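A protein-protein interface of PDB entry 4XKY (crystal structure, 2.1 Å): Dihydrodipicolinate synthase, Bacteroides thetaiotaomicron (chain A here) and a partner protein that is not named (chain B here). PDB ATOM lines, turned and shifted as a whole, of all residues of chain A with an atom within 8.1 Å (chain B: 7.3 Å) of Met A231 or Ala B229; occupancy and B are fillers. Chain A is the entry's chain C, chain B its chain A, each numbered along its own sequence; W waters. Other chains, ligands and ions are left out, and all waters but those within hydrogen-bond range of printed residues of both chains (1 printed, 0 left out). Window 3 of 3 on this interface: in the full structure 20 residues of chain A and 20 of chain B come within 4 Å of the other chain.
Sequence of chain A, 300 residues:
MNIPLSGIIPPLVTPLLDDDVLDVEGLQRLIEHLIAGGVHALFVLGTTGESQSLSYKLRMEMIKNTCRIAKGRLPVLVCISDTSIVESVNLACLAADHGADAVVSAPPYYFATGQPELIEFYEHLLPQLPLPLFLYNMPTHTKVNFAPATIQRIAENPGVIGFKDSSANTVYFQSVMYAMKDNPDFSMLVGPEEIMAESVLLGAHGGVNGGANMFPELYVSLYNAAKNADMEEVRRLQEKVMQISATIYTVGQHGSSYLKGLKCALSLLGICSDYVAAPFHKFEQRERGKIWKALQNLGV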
ATOM      1  N   ALA A 197     -17.217 -21.869  32.840  1.00  0.00           N
ATOM      2  CA  ALA A 197     -17.656 -21.557  31.483  1.00  0.00           C
ATOM      3  C   ALA A 197     -18.679 -22.549  30.970  1.00  0.00           C
ATOM      4  O   ALA A 197     -19.753 -22.147  30.518  1.00  0.00           O
ATOM      5  CB  ALA A 197     -16.476 -21.507  30.530  1.00  0.00           C
ATOM      6  N   GLU A 198     -18.357 -23.842  31.037  1.00  0.00           N
ATOM      7  CA  GLU A 198     -19.257 -24.841  30.475  1.00  0.00           C
ATOM      8  C   GLU A 198     -20.573 -24.861  31.218  1.00  0.00           C
ATOM      9  O   GLU A 198     -21.597 -25.112  30.610  1.00  0.00           O
ATOM     10  CB  GLU A 198     -18.644 -26.247  30.418  1.00  0.00           C
ATOM     11  CG  GLU A 198     -18.527 -26.982  31.738  1.00  0.00           C
ATOM     12  CD  GLU A 198     -17.608 -28.191  31.651  1.00  0.00           C
ATOM     13  OE1 GLU A 198     -18.095 -29.313  31.833  1.00  0.00           O
ATOM     14  OE2 GLU A 198     -16.398 -28.027  31.420  1.00  0.00           O
ATOM     15  N   LEU A 201     -22.561 -21.707  30.146  1.00  0.00           N
ATOM     16  CA  LEU A 201     -23.129 -21.966  28.803  1.00  0.00           C
ATOM     17  C   LEU A 201     -24.475 -22.690  28.864  1.00  0.00           C
ATOM     18  O   LEU A 201     -25.364 -22.438  28.050  1.00  0.00           O
ATOM     19  CB  LEU A 201     -22.179 -22.812  27.957  1.00  0.00           C
ATOM     20  CG  LEU A 201     -21.060 -22.028  27.284  1.00  0.00           C
ATOM     21  CD1 LEU A 201     -19.914 -22.922  26.842  1.00  0.00           C
ATOM     22  CD2 LEU A 201     -21.608 -21.277  26.094  1.00  0.00           C
ATOM     23  N   LEU A 222     -14.802 -14.108  30.916  1.00  0.00           N
ATOM     24  CA  LEU A 222     -15.151 -15.464  30.544  1.00  0.00           C
ATOM     25  C   LEU A 222     -16.614 -15.745  30.835  1.00  0.00           C
ATOM     26  O   LEU A 222     -17.286 -16.392  30.040  1.00  0.00           O
ATOM     27  CB  LEU A 222     -14.264 -16.458  31.280  1.00  0.00           C
ATOM     28  CG  LEU A 222     -14.548 -17.930  31.035  1.00  0.00           C
ATOM     29  CD1 LEU A 222     -14.623 -18.294  29.563  1.00  0.00           C
ATOM     30  CD2 LEU A 222     -13.457 -18.720  31.726  1.00  0.00           C
ATOM     31  N   ALA A 225     -18.668 -14.000  28.143  1.00  0.00           N
ATOM     32  CA  ALA A 225     -18.519 -14.763  26.904  1.00  0.00           C
ATOM     33  C   ALA A 225     -19.423 -16.010  26.930  1.00  0.00           C
ATOM     34  O   ALA A 225     -20.131 -16.313  25.966  1.00  0.00           O
ATOM     35  CB  ALA A 225     -17.063 -15.167  26.700  1.00  0.00           C
ATOM     36  N   ALA A 226     -19.391 -16.710  28.056  1.00  0.00           N
ATOM     37  CA  ALA A 226     -20.138 -17.946  28.213  1.00  0.00           C
ATOM     38  C   ALA A 226     -21.617 -17.644  28.201  1.00  0.00           C
ATOM     39  O   ALA A 226     -22.384 -18.303  27.516  1.00  0.00           O
ATOM     40  CB  ALA A 226     -19.751 -18.649  29.502  1.00  0.00           C
ATOM     41  N   ASN A 228     -23.181 -15.196  26.720  1.00  0.00           N
ATOM     42  CA  ASN A 228     -23.586 -14.846  25.350  1.00  0.00           C
ATOM     43  C   ASN A 228     -23.092 -15.835  24.285  1.00  0.00           C
ATOM     44  O   ASN A 228     -23.244 -15.575  23.088  1.00  0.00           O
ATOM     45  CB  ASN A 228     -23.087 -13.437  24.991  1.00  0.00           C
ATOM     46  CG  ASN A 228     -23.305 -12.431  26.110  1.00  0.00           C
ATOM     47  OD1 ASN A 228     -22.389 -11.701  26.496  1.00  0.00           O
ATOM     48  ND2 ASN A 228     -24.516 -12.395  26.643  1.00  0.00           N
ATOM     49  N   ALA A 229     -22.512 -16.960  24.712  1.00  0.00           N
ATOM     50  CA  ALA A 229     -21.980 -17.984  23.792  1.00  0.00           C
ATOM     51  C   ALA A 229     -21.132 -17.383  22.664  1.00  0.00           C
ATOM     52  O   ALA A 229     -21.318 -17.697  21.483  1.00  0.00           O
ATOM     53  CB  ALA A 229     -23.105 -18.824  23.211  1.00  0.00           C
ATOM     54  N   ASP A 230     -20.215 -16.504  23.046  1.00  0.00           N
ATOM     55  CA  ASP A 230     -19.150 -16.059  22.155  1.00  0.00           C
ATOM     56  C   ASP A 230     -18.016 -17.102  22.263  1.00  0.00           C
ATOM     57  O   ASP A 230     -17.082 -16.989  23.064  1.00  0.00           O
ATOM     58  CB  ASP A 230     -18.713 -14.632  22.522  1.00  0.00           C
ATOM     59  CG  ASP A 230     -17.456 -14.174  21.779  1.00  0.00           C
ATOM     60  OD1 ASP A 230     -16.916 -14.925  20.934  1.00  0.00           O
ATOM     61  OD2 ASP A 230     -17.001 -13.045  22.067  1.00  0.00           O
ATOM     62  N   MET A 231     -18.131 -18.122  21.427  1.00  0.00           N
ATOM     63  CA  MET A 231     -17.353 -19.350  21.580  1.00  0.00           C
ATOM     64  C   MET A 231     -15.862 -19.156  21.378  1.00  0.00           C
ATOM     65  O   MET A 231     -15.084 -19.875  22.001  1.00  0.00           O
ATOM     66  CB  MET A 231     -17.908 -20.447  20.649  1.00  0.00           C
ATOM     67  CG  MET A 231     -19.335 -20.851  21.000  1.00  0.00           C
ATOM     68  SD  MET A 231     -19.545 -21.299  22.740  1.00  0.00           S
ATOM     69  CE  MET A 231     -18.281 -22.550  22.922  1.00  0.00           C
ATOM     70  N   GLU A 232     -15.459 -18.191  20.544  1.00  0.00           N
ATOM     71  CA  GLU A 232     -14.029 -17.918  20.337  1.00  0.00           C
ATOM     72  C   GLU A 232     -13.421 -17.317  21.598  1.00  0.00           C
ATOM     73  O   GLU A 232     -12.309 -17.652  21.988  1.00  0.00           O
ATOM     74  CB  GLU A 232     -13.796 -16.977  19.146  1.00  0.00           C
ATOM     75  N   GLU A 233     -14.157 -16.418  22.231  1.00  0.00           N
ATOM     76  CA  GLU A 233     -13.717 -15.841  23.491  1.00  0.00           C
ATOM     77  C   GLU A 233     -13.748 -16.883  24.607  1.00  0.00           C
ATOM     78  O   GLU A 233     -12.823 -16.937  25.419  1.00  0.00           O
ATOM     79  CB  GLU A 233     -14.564 -14.626  23.874  1.00  0.00           C
ATOM     80  CG  GLU A 233     -14.148 -13.353  23.160  1.00  0.00           C
ATOM     81  CD  GLU A 233     -12.709 -12.984  23.456  1.00  0.00           C
ATOM     82  OE1 GLU A 233     -11.836 -13.282  22.611  1.00  0.00           O
ATOM     83  OE2 GLU A 233     -12.453 -12.444  24.554  1.00  0.00           O
ATOM     84  N   VAL A 234     -14.793 -17.713  24.638  1.00  0.00           N
ATOM     85  CA  VAL A 234     -14.852 -18.771  25.637  1.00  0.00           C
ATOM     86  C   VAL A 234     -13.615 -19.659  25.538  1.00  0.00           C
ATOM     87  O   VAL A 234     -12.980 -19.937  26.546  1.00  0.00           O
ATOM     88  CB  VAL A 234     -16.132 -19.631  25.552  1.00  0.00           C
ATOM     89  CG1 VAL A 234     -15.978 -20.927  26.353  1.00  0.00           C
ATOM     90  CG2 VAL A 234     -17.312 -18.843  26.084  1.00  0.00           C
ATOM     91  N   ARG A 235     -13.268 -20.083  24.328  1.00  0.00           N
ATOM     92  CA  ARG A 235     -12.111 -20.963  24.120  1.00  0.00           C
ATOM     93  C   ARG A 235     -10.773 -20.299  24.470  1.00  0.00           C
ATOM     94  O   ARG A 235      -9.923 -20.915  25.107  1.00  0.00           O
ATOM     95  CB  ARG A 235     -12.073 -21.475  22.686  1.00  0.00           C
ATOM     96  CG  ARG A 235     -12.997 -22.649  22.427  1.00  0.00           C
ATOM     97  CD  ARG A 235     -12.757 -23.211  21.031  1.00  0.00           C
ATOM     98  NE  ARG A 235     -13.166 -22.281  19.969  1.00  0.00           N
ATOM     99  CZ  ARG A 235     -14.358 -22.278  19.366  1.00  0.00           C
ATOM    100  NH1 ARG A 235     -14.608 -21.385  18.417  1.00  0.00           N
ATOM    101  NH2 ARG A 235     -15.308 -23.153  19.694  1.00  0.00           N
ATOM    102  N   ARG A 236     -10.589 -19.056  24.035  1.00  0.00           N
ATOM    103  CA  ARG A 236      -9.368 -18.304  24.324  1.00  0.00           C
ATOM    104  C   ARG A 236      -9.245 -18.081  25.836  1.00  0.00           C
ATOM    105  O   ARG A 236      -8.201 -18.339  26.422  1.00  0.00           O
ATOM    106  CB  ARG A 236      -9.385 -16.973  23.551  1.00  0.00           C
ATOM    107  CG  ARG A 236      -8.193 -16.058  23.773  1.00  0.00           C
ATOM    108  CD  ARG A 236      -8.339 -14.783  22.965  1.00  0.00           C
ATOM    109  NE  ARG A 236      -9.166 -13.796  23.648  1.00  0.00           N
ATOM    110  CZ  ARG A 236      -8.754 -13.041  24.662  1.00  0.00           C
ATOM    111  NH1 ARG A 236      -7.523 -13.155  25.159  1.00  0.00           N
ATOM    112  NH2 ARG A 236      -9.591 -12.172  25.202  1.00  0.00           N
ATOM    113  N   LEU A 237     -10.333 -17.659  26.473  1.00  0.00           N
ATOM    114  CA  LEU A 237     -10.273 -17.346  27.902  1.00  0.00           C
ATOM    115  C   LEU A 237     -10.253 -18.586  28.772  1.00  0.00           C
ATOM    116  O   LEU A 237      -9.581 -18.586  29.794  1.00  0.00           O
ATOM    117  CB  LEU A 237     -11.397 -16.406  28.321  1.00  0.00           C
ATOM    118  CG  LEU A 237     -11.359 -15.029  27.653  1.00  0.00           C
ATOM    119  CD1 LEU A 237     -12.567 -14.232  28.106  1.00  0.00           C
ATOM    120  CD2 LEU A 237     -10.082 -14.257  27.964  1.00  0.00           C
ATOM    121  N   GLN A 238     -10.958 -19.641  28.371  1.00  0.00           N
ATOM    122  CA  GLN A 238     -10.855 -20.914  29.084  1.00  0.00           C
ATOM    123  C   GLN A 238      -9.416 -21.432  29.150  1.00  0.00           C
ATOM    124  O   GLN A 238      -8.986 -21.921  30.197  1.00  0.00           O
ATOM    125  CB  GLN A 238     -11.771 -21.975  28.480  1.00  0.00           C
ATOM    126  CG  GLN A 238     -11.661 -23.363  29.091  1.00  0.00           C
ATOM    127  CD  GLN A 238     -12.241 -23.506  30.490  1.00  0.00           C
ATOM    128  OE1 GLN A 238     -12.202 -24.605  31.056  1.00  0.00           O
ATOM    129  NE2 GLN A 238     -12.786 -22.428  31.057  1.00  0.00           N
ATOM    130  N   VAL B 200     -18.621 -31.346  24.826  1.00  0.00           N
ATOM    131  CA  VAL B 200     -18.387 -31.174  23.388  1.00  0.00           C
ATOM    132  C   VAL B 200     -18.289 -29.689  23.031  1.00  0.00           C
ATOM    133  O   VAL B 200     -17.436 -29.291  22.246  1.00  0.00           O
ATOM    134  CB  VAL B 200     -19.450 -31.888  22.525  1.00  0.00           C
ATOM    135  CG1 VAL B 200     -19.306 -31.529  21.051  1.00  0.00           C
ATOM    136  CG2 VAL B 200     -19.300 -33.389  22.664  1.00  0.00           C
ATOM    137  N   LEU B 201     -19.135 -28.864  23.633  1.00  0.00           N
ATOM    138  CA  LEU B 201     -19.091 -27.422  23.388  1.00  0.00           C
ATOM    139  C   LEU B 201     -17.699 -26.863  23.549  1.00  0.00           C
ATOM    140  O   LEU B 201     -17.297 -25.945  22.828  1.00  0.00           O
ATOM    141  CB  LEU B 201     -20.031 -26.676  24.329  1.00  0.00           C
ATOM    142  CG  LEU B 201     -21.454 -26.554  23.808  1.00  0.00           C
ATOM    143  CD1 LEU B 201     -22.381 -26.141  24.936  1.00  0.00           C
ATOM    144  CD2 LEU B 201     -21.530 -25.545  22.670  1.00  0.00           C
ATOM    145  N   LEU B 202     -16.989 -27.409  24.526  1.00  0.00           N
ATOM    146  CA  LEU B 202     -15.617 -27.029  24.825  1.00  0.00           C
ATOM    147  C   LEU B 202     -14.603 -27.981  24.205  1.00  0.00           C
ATOM    148  O   LEU B 202     -13.503 -28.123  24.714  1.00  0.00           O
ATOM    149  CB  LEU B 202     -15.414 -27.012  26.339  1.00  0.00           C
ATOM    150  CG  LEU B 202     -15.656 -25.675  27.003  1.00  0.00           C
ATOM    151  CD1 LEU B 202     -17.097 -25.229  26.870  1.00  0.00           C
ATOM    152  CD2 LEU B 202     -15.272 -25.804  28.467  1.00  0.00           C
ATOM    153  N   GLY B 203     -14.971 -28.644  23.116  1.00  0.00           N
ATOM    154  CA  GLY B 203     -13.990 -29.366  22.300  1.00  0.00           C
ATOM    155  C   GLY B 203     -13.780 -30.852  22.554  1.00  0.00           C
ATOM    156  O   GLY B 203     -12.917 -31.444  21.914  1.00  0.00           O
ATOM    157  N   TYR B 223     -25.064 -34.017  19.910  1.00  0.00           N
ATOM    158  CA  TYR B 223     -23.635 -33.922  19.633  1.00  0.00           C
ATOM    159  C   TYR B 223     -23.324 -32.842  18.569  1.00  0.00           C
ATOM    160  O   TYR B 223     -22.394 -32.025  18.740  1.00  0.00           O
ATOM    161  CB  TYR B 223     -23.050 -35.266  19.185  1.00  0.00           C
ATOM    162  CG  TYR B 223     -21.671 -35.102  18.577  1.00  0.00           C
ATOM    163  CD1 TYR B 223     -20.549 -34.915  19.392  1.00  0.00           C
ATOM    164  CD2 TYR B 223     -21.485 -35.089  17.185  1.00  0.00           C
ATOM    165  CE1 TYR B 223     -19.281 -34.749  18.846  1.00  0.00           C
ATOM    166  CE2 TYR B 223     -20.217 -34.917  16.628  1.00  0.00           C
ATOM    167  CZ  TYR B 223     -19.121 -34.734  17.459  1.00  0.00           C
ATOM    168  OH  TYR B 223     -17.854 -34.557  16.920  1.00  0.00           O
ATOM    169  N   ASN B 224     -24.088 -32.870  17.478  1.00  0.00           N
ATOM    170  CA  ASN B 224     -23.930 -31.933  16.348  1.00  0.00           C
ATOM    171  C   ASN B 224     -24.267 -30.475  16.696  1.00  0.00           C
ATOM    172  O   ASN B 224     -23.570 -29.548  16.267  1.00  0.00           O
ATOM    173  CB  ASN B 224     -24.782 -32.422  15.158  1.00  0.00           C
ATOM    174  CG  ASN B 224     -24.158 -33.617  14.452  1.00  0.00           C
ATOM    175  OD1 ASN B 224     -22.966 -33.631  14.206  1.00  0.00           O
ATOM    176  ND2 ASN B 224     -24.953 -34.608  14.115  1.00  0.00           N
ATOM    177  N   ALA B 225     -25.336 -30.295  17.473  1.00  0.00           N
ATOM    178  CA  ALA B 225     -25.702 -28.996  18.015  1.00  0.00           C
ATOM    179  C   ALA B 225     -24.623 -28.470  18.972  1.00  0.00           C
ATOM    180  O   ALA B 225     -24.376 -27.264  18.993  1.00  0.00           O
ATOM    181  CB  ALA B 225     -27.032 -29.078  18.742  1.00  0.00           C
ATOM    182  N   ALA B 226     -23.994 -29.343  19.771  1.00  0.00           N
ATOM    183  CA  ALA B 226     -22.914 -28.879  20.685  1.00  0.00           C
ATOM    184  C   ALA B 226     -21.668 -28.523  19.881  1.00  0.00           C
ATOM    185  O   ALA B 226     -20.991 -27.524  20.149  1.00  0.00           O
ATOM    186  CB  ALA B 226     -22.582 -29.917  21.754  1.00  0.00           C
ATOM    187  N   LYS B 227     -21.414 -29.339  18.861  1.00  0.00           N
ATOM    188  CA  LYS B 227     -20.266 -29.188  17.976  1.00  0.00           C
ATOM    189  C   LYS B 227     -20.261 -27.865  17.278  1.00  0.00           C
ATOM    190  O   LYS B 227     -19.226 -27.216  17.161  1.00  0.00           O
ATOM    191  CB  LYS B 227     -20.271 -30.256  16.892  1.00  0.00           C
ATOM    192  CG  LYS B 227     -18.926 -30.354  16.212  1.00  0.00           C
ATOM    193  CD  LYS B 227     -18.940 -31.361  15.092  1.00  0.00           C
ATOM    194  CE  LYS B 227     -17.602 -31.330  14.376  1.00  0.00           C
ATOM    195  NZ  LYS B 227     -17.685 -31.984  13.046  1.00  0.00           N
ATOM    196  N   ASN B 228     -21.430 -27.498  16.786  1.00  0.00           N
ATOM    197  CA  ASN B 228     -21.605 -26.276  16.031  1.00  0.00           C
ATOM    198  C   ASN B 228     -22.082 -25.126  16.890  1.00  0.00           C
ATOM    199  O   ASN B 228     -22.376 -24.063  16.378  1.00  0.00           O
ATOM    200  CB  ASN B 228     -22.609 -26.546  14.917  1.00  0.00           C
ATOM    201  CG  ASN B 228     -22.148 -27.657  13.998  1.00  0.00           C
ATOM    202  OD1 ASN B 228     -21.015 -27.638  13.510  1.00  0.00           O
ATOM    203  ND2 ASN B 228     -23.011 -28.636  13.764  1.00  0.00           N
ATOM    204  N   ALA B 229     -22.190 -25.341  18.197  1.00  0.00           N
ATOM    205  CA  ALA B 229     -22.638 -24.291  19.100  1.00  0.00           C
ATOM    206  C   ALA B 229     -24.003 -23.715  18.670  1.00  0.00           C
ATOM    207  O   ALA B 229     -24.244 -22.514  18.777  1.00  0.00           O
ATOM    208  CB  ALA B 229     -21.579 -23.191  19.198  1.00  0.00           C
ATOM    209  N   ASP B 230     -24.891 -24.578  18.183  1.00  0.00           N
ATOM    210  CA  ASP B 230     -26.292 -24.203  17.982  1.00  0.00           C
ATOM    211  C   ASP B 230     -27.033 -24.251  19.339  1.00  0.00           C
ATOM    212  O   ASP B 230     -27.636 -25.257  19.727  1.00  0.00           O
ATOM    213  CB  ASP B 230     -26.930 -25.110  16.924  1.00  0.00           C
ATOM    214  CG  ASP B 230     -28.364 -24.763  16.646  1.00  0.00           C
ATOM    215  OD1 ASP B 230     -28.924 -23.876  17.316  1.00  0.00           O
ATOM    216  OD2 ASP B 230     -28.941 -25.392  15.742  1.00  0.00           O
ATOM    217  N   MET B 231     -26.977 -23.135  20.048  1.00  0.00           N
ATOM    218  CA  MET B 231     -27.345 -23.098  21.453  1.00  0.00           C
ATOM    219  C   MET B 231     -28.824 -23.396  21.744  1.00  0.00           C
ATOM    220  O   MET B 231     -29.119 -24.091  22.707  1.00  0.00           O
ATOM    221  CB  MET B 231     -26.927 -21.753  22.067  1.00  0.00           C
ATOM    222  CG  MET B 231     -25.417 -21.548  22.155  1.00  0.00           C
ATOM    223  SD  MET B 231     -24.453 -22.923  22.875  1.00  0.00           S
ATOM    224  CE  MET B 231     -25.181 -23.062  24.499  1.00  0.00           C
ATOM    225  N   GLU B 232     -29.745 -22.865  20.942  1.00  0.00           N
ATOM    226  CA  GLU B 232     -31.194 -23.130  21.131  1.00  0.00           C
ATOM    227  C   GLU B 232     -31.480 -24.626  21.093  1.00  0.00           C
ATOM    228  O   GLU B 232     -32.222 -25.175  21.923  1.00  0.00           O
ATOM    229  CB  GLU B 232     -32.023 -22.422  20.053  1.00  0.00           C
ATOM    230  N   GLU B 233     -30.867 -25.275  20.110  1.00  0.00           N
ATOM    231  CA  GLU B 233     -30.979 -26.716  19.929  1.00  0.00           C
ATOM    232  C   GLU B 233     -30.241 -27.510  21.038  1.00  0.00           C
ATOM    233  O   GLU B 233     -30.758 -28.530  21.531  1.00  0.00           O
ATOM    234  CB  GLU B 233     -30.484 -27.083  18.528  1.00  0.00           C
ATOM    235  CG  GLU B 233     -31.029 -28.385  17.971  1.00  0.00           C
ATOM    236  CD  GLU B 233     -32.532 -28.391  17.727  1.00  0.00           C
ATOM    237  OE1 GLU B 233     -33.263 -27.410  18.006  1.00  0.00           O
ATOM    238  OE2 GLU B 233     -33.004 -29.430  17.257  1.00  0.00           O
ATOM    239  N   VAL B 234     -29.054 -27.063  21.447  1.00  0.00           N
ATOM    240  CA  VAL B 234     -28.394 -27.674  22.623  1.00  0.00           C
ATOM    241  C   VAL B 234     -29.371 -27.660  23.818  1.00  0.00           C
ATOM    242  O   VAL B 234     -29.621 -28.695  24.447  1.00  0.00           O
ATOM    243  CB  VAL B 234     -27.077 -26.961  23.003  1.00  0.00           C
ATOM    244  CG1 VAL B 234     -26.577 -27.415  24.355  1.00  0.00           C
ATOM    245  CG2 VAL B 234     -26.005 -27.231  21.974  1.00  0.00           C
HETATM  246  O   HOH W   1     -14.931 -24.976  21.743  1.00  0.00           O
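Glu A198 touches Leu B202 (OE2 to CD2, 3.9 Å). Leu A201 touches Leu B202 (CD1 to CD1, 3.6 Å). Met B231 touches Leu A201. CB of Ala A229 touches CG of Met B231 (3.7 Å). O of Leu B201 touches CE of Met A231 (3.5 Å). Ala B229 touches Met A231.
Of the printed residues of chain B, Leu A201 touches Leu B202 (3.6 Å) and Met B231 (3.6 Å). Of the printed residues of chain A, Leu B201 touches Met A231 (3.5 Å). Of the printed residues of chain A, Leu B202 touches Glu A198 (3.9 Å) and Leu A201 (3.6 Å). Asp B230 touches none of the printed residues of chain A. Of the printed residues of chain A, Met B231 touches Leu A201 and Ala A229.
Of the 17 printed residues of chain A, 4 touch a printed residue of chain B. Printed residues of chain A that touch a printed residue of chain B: Glu A198, Leu A201, Ala A229 and Met A231. Hydrophobic or aromatic side chains of chain A that line the printed part of chain B: Leu A201, Ala A229 and Met A231. Among the printed residues, 6 pairs touch across the chains.
Water W1 bridges the guanidinium group of Arg A235 (2.8 Å) and the backbone carbonyl oxygen of Leu B201 (2.8 Å).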
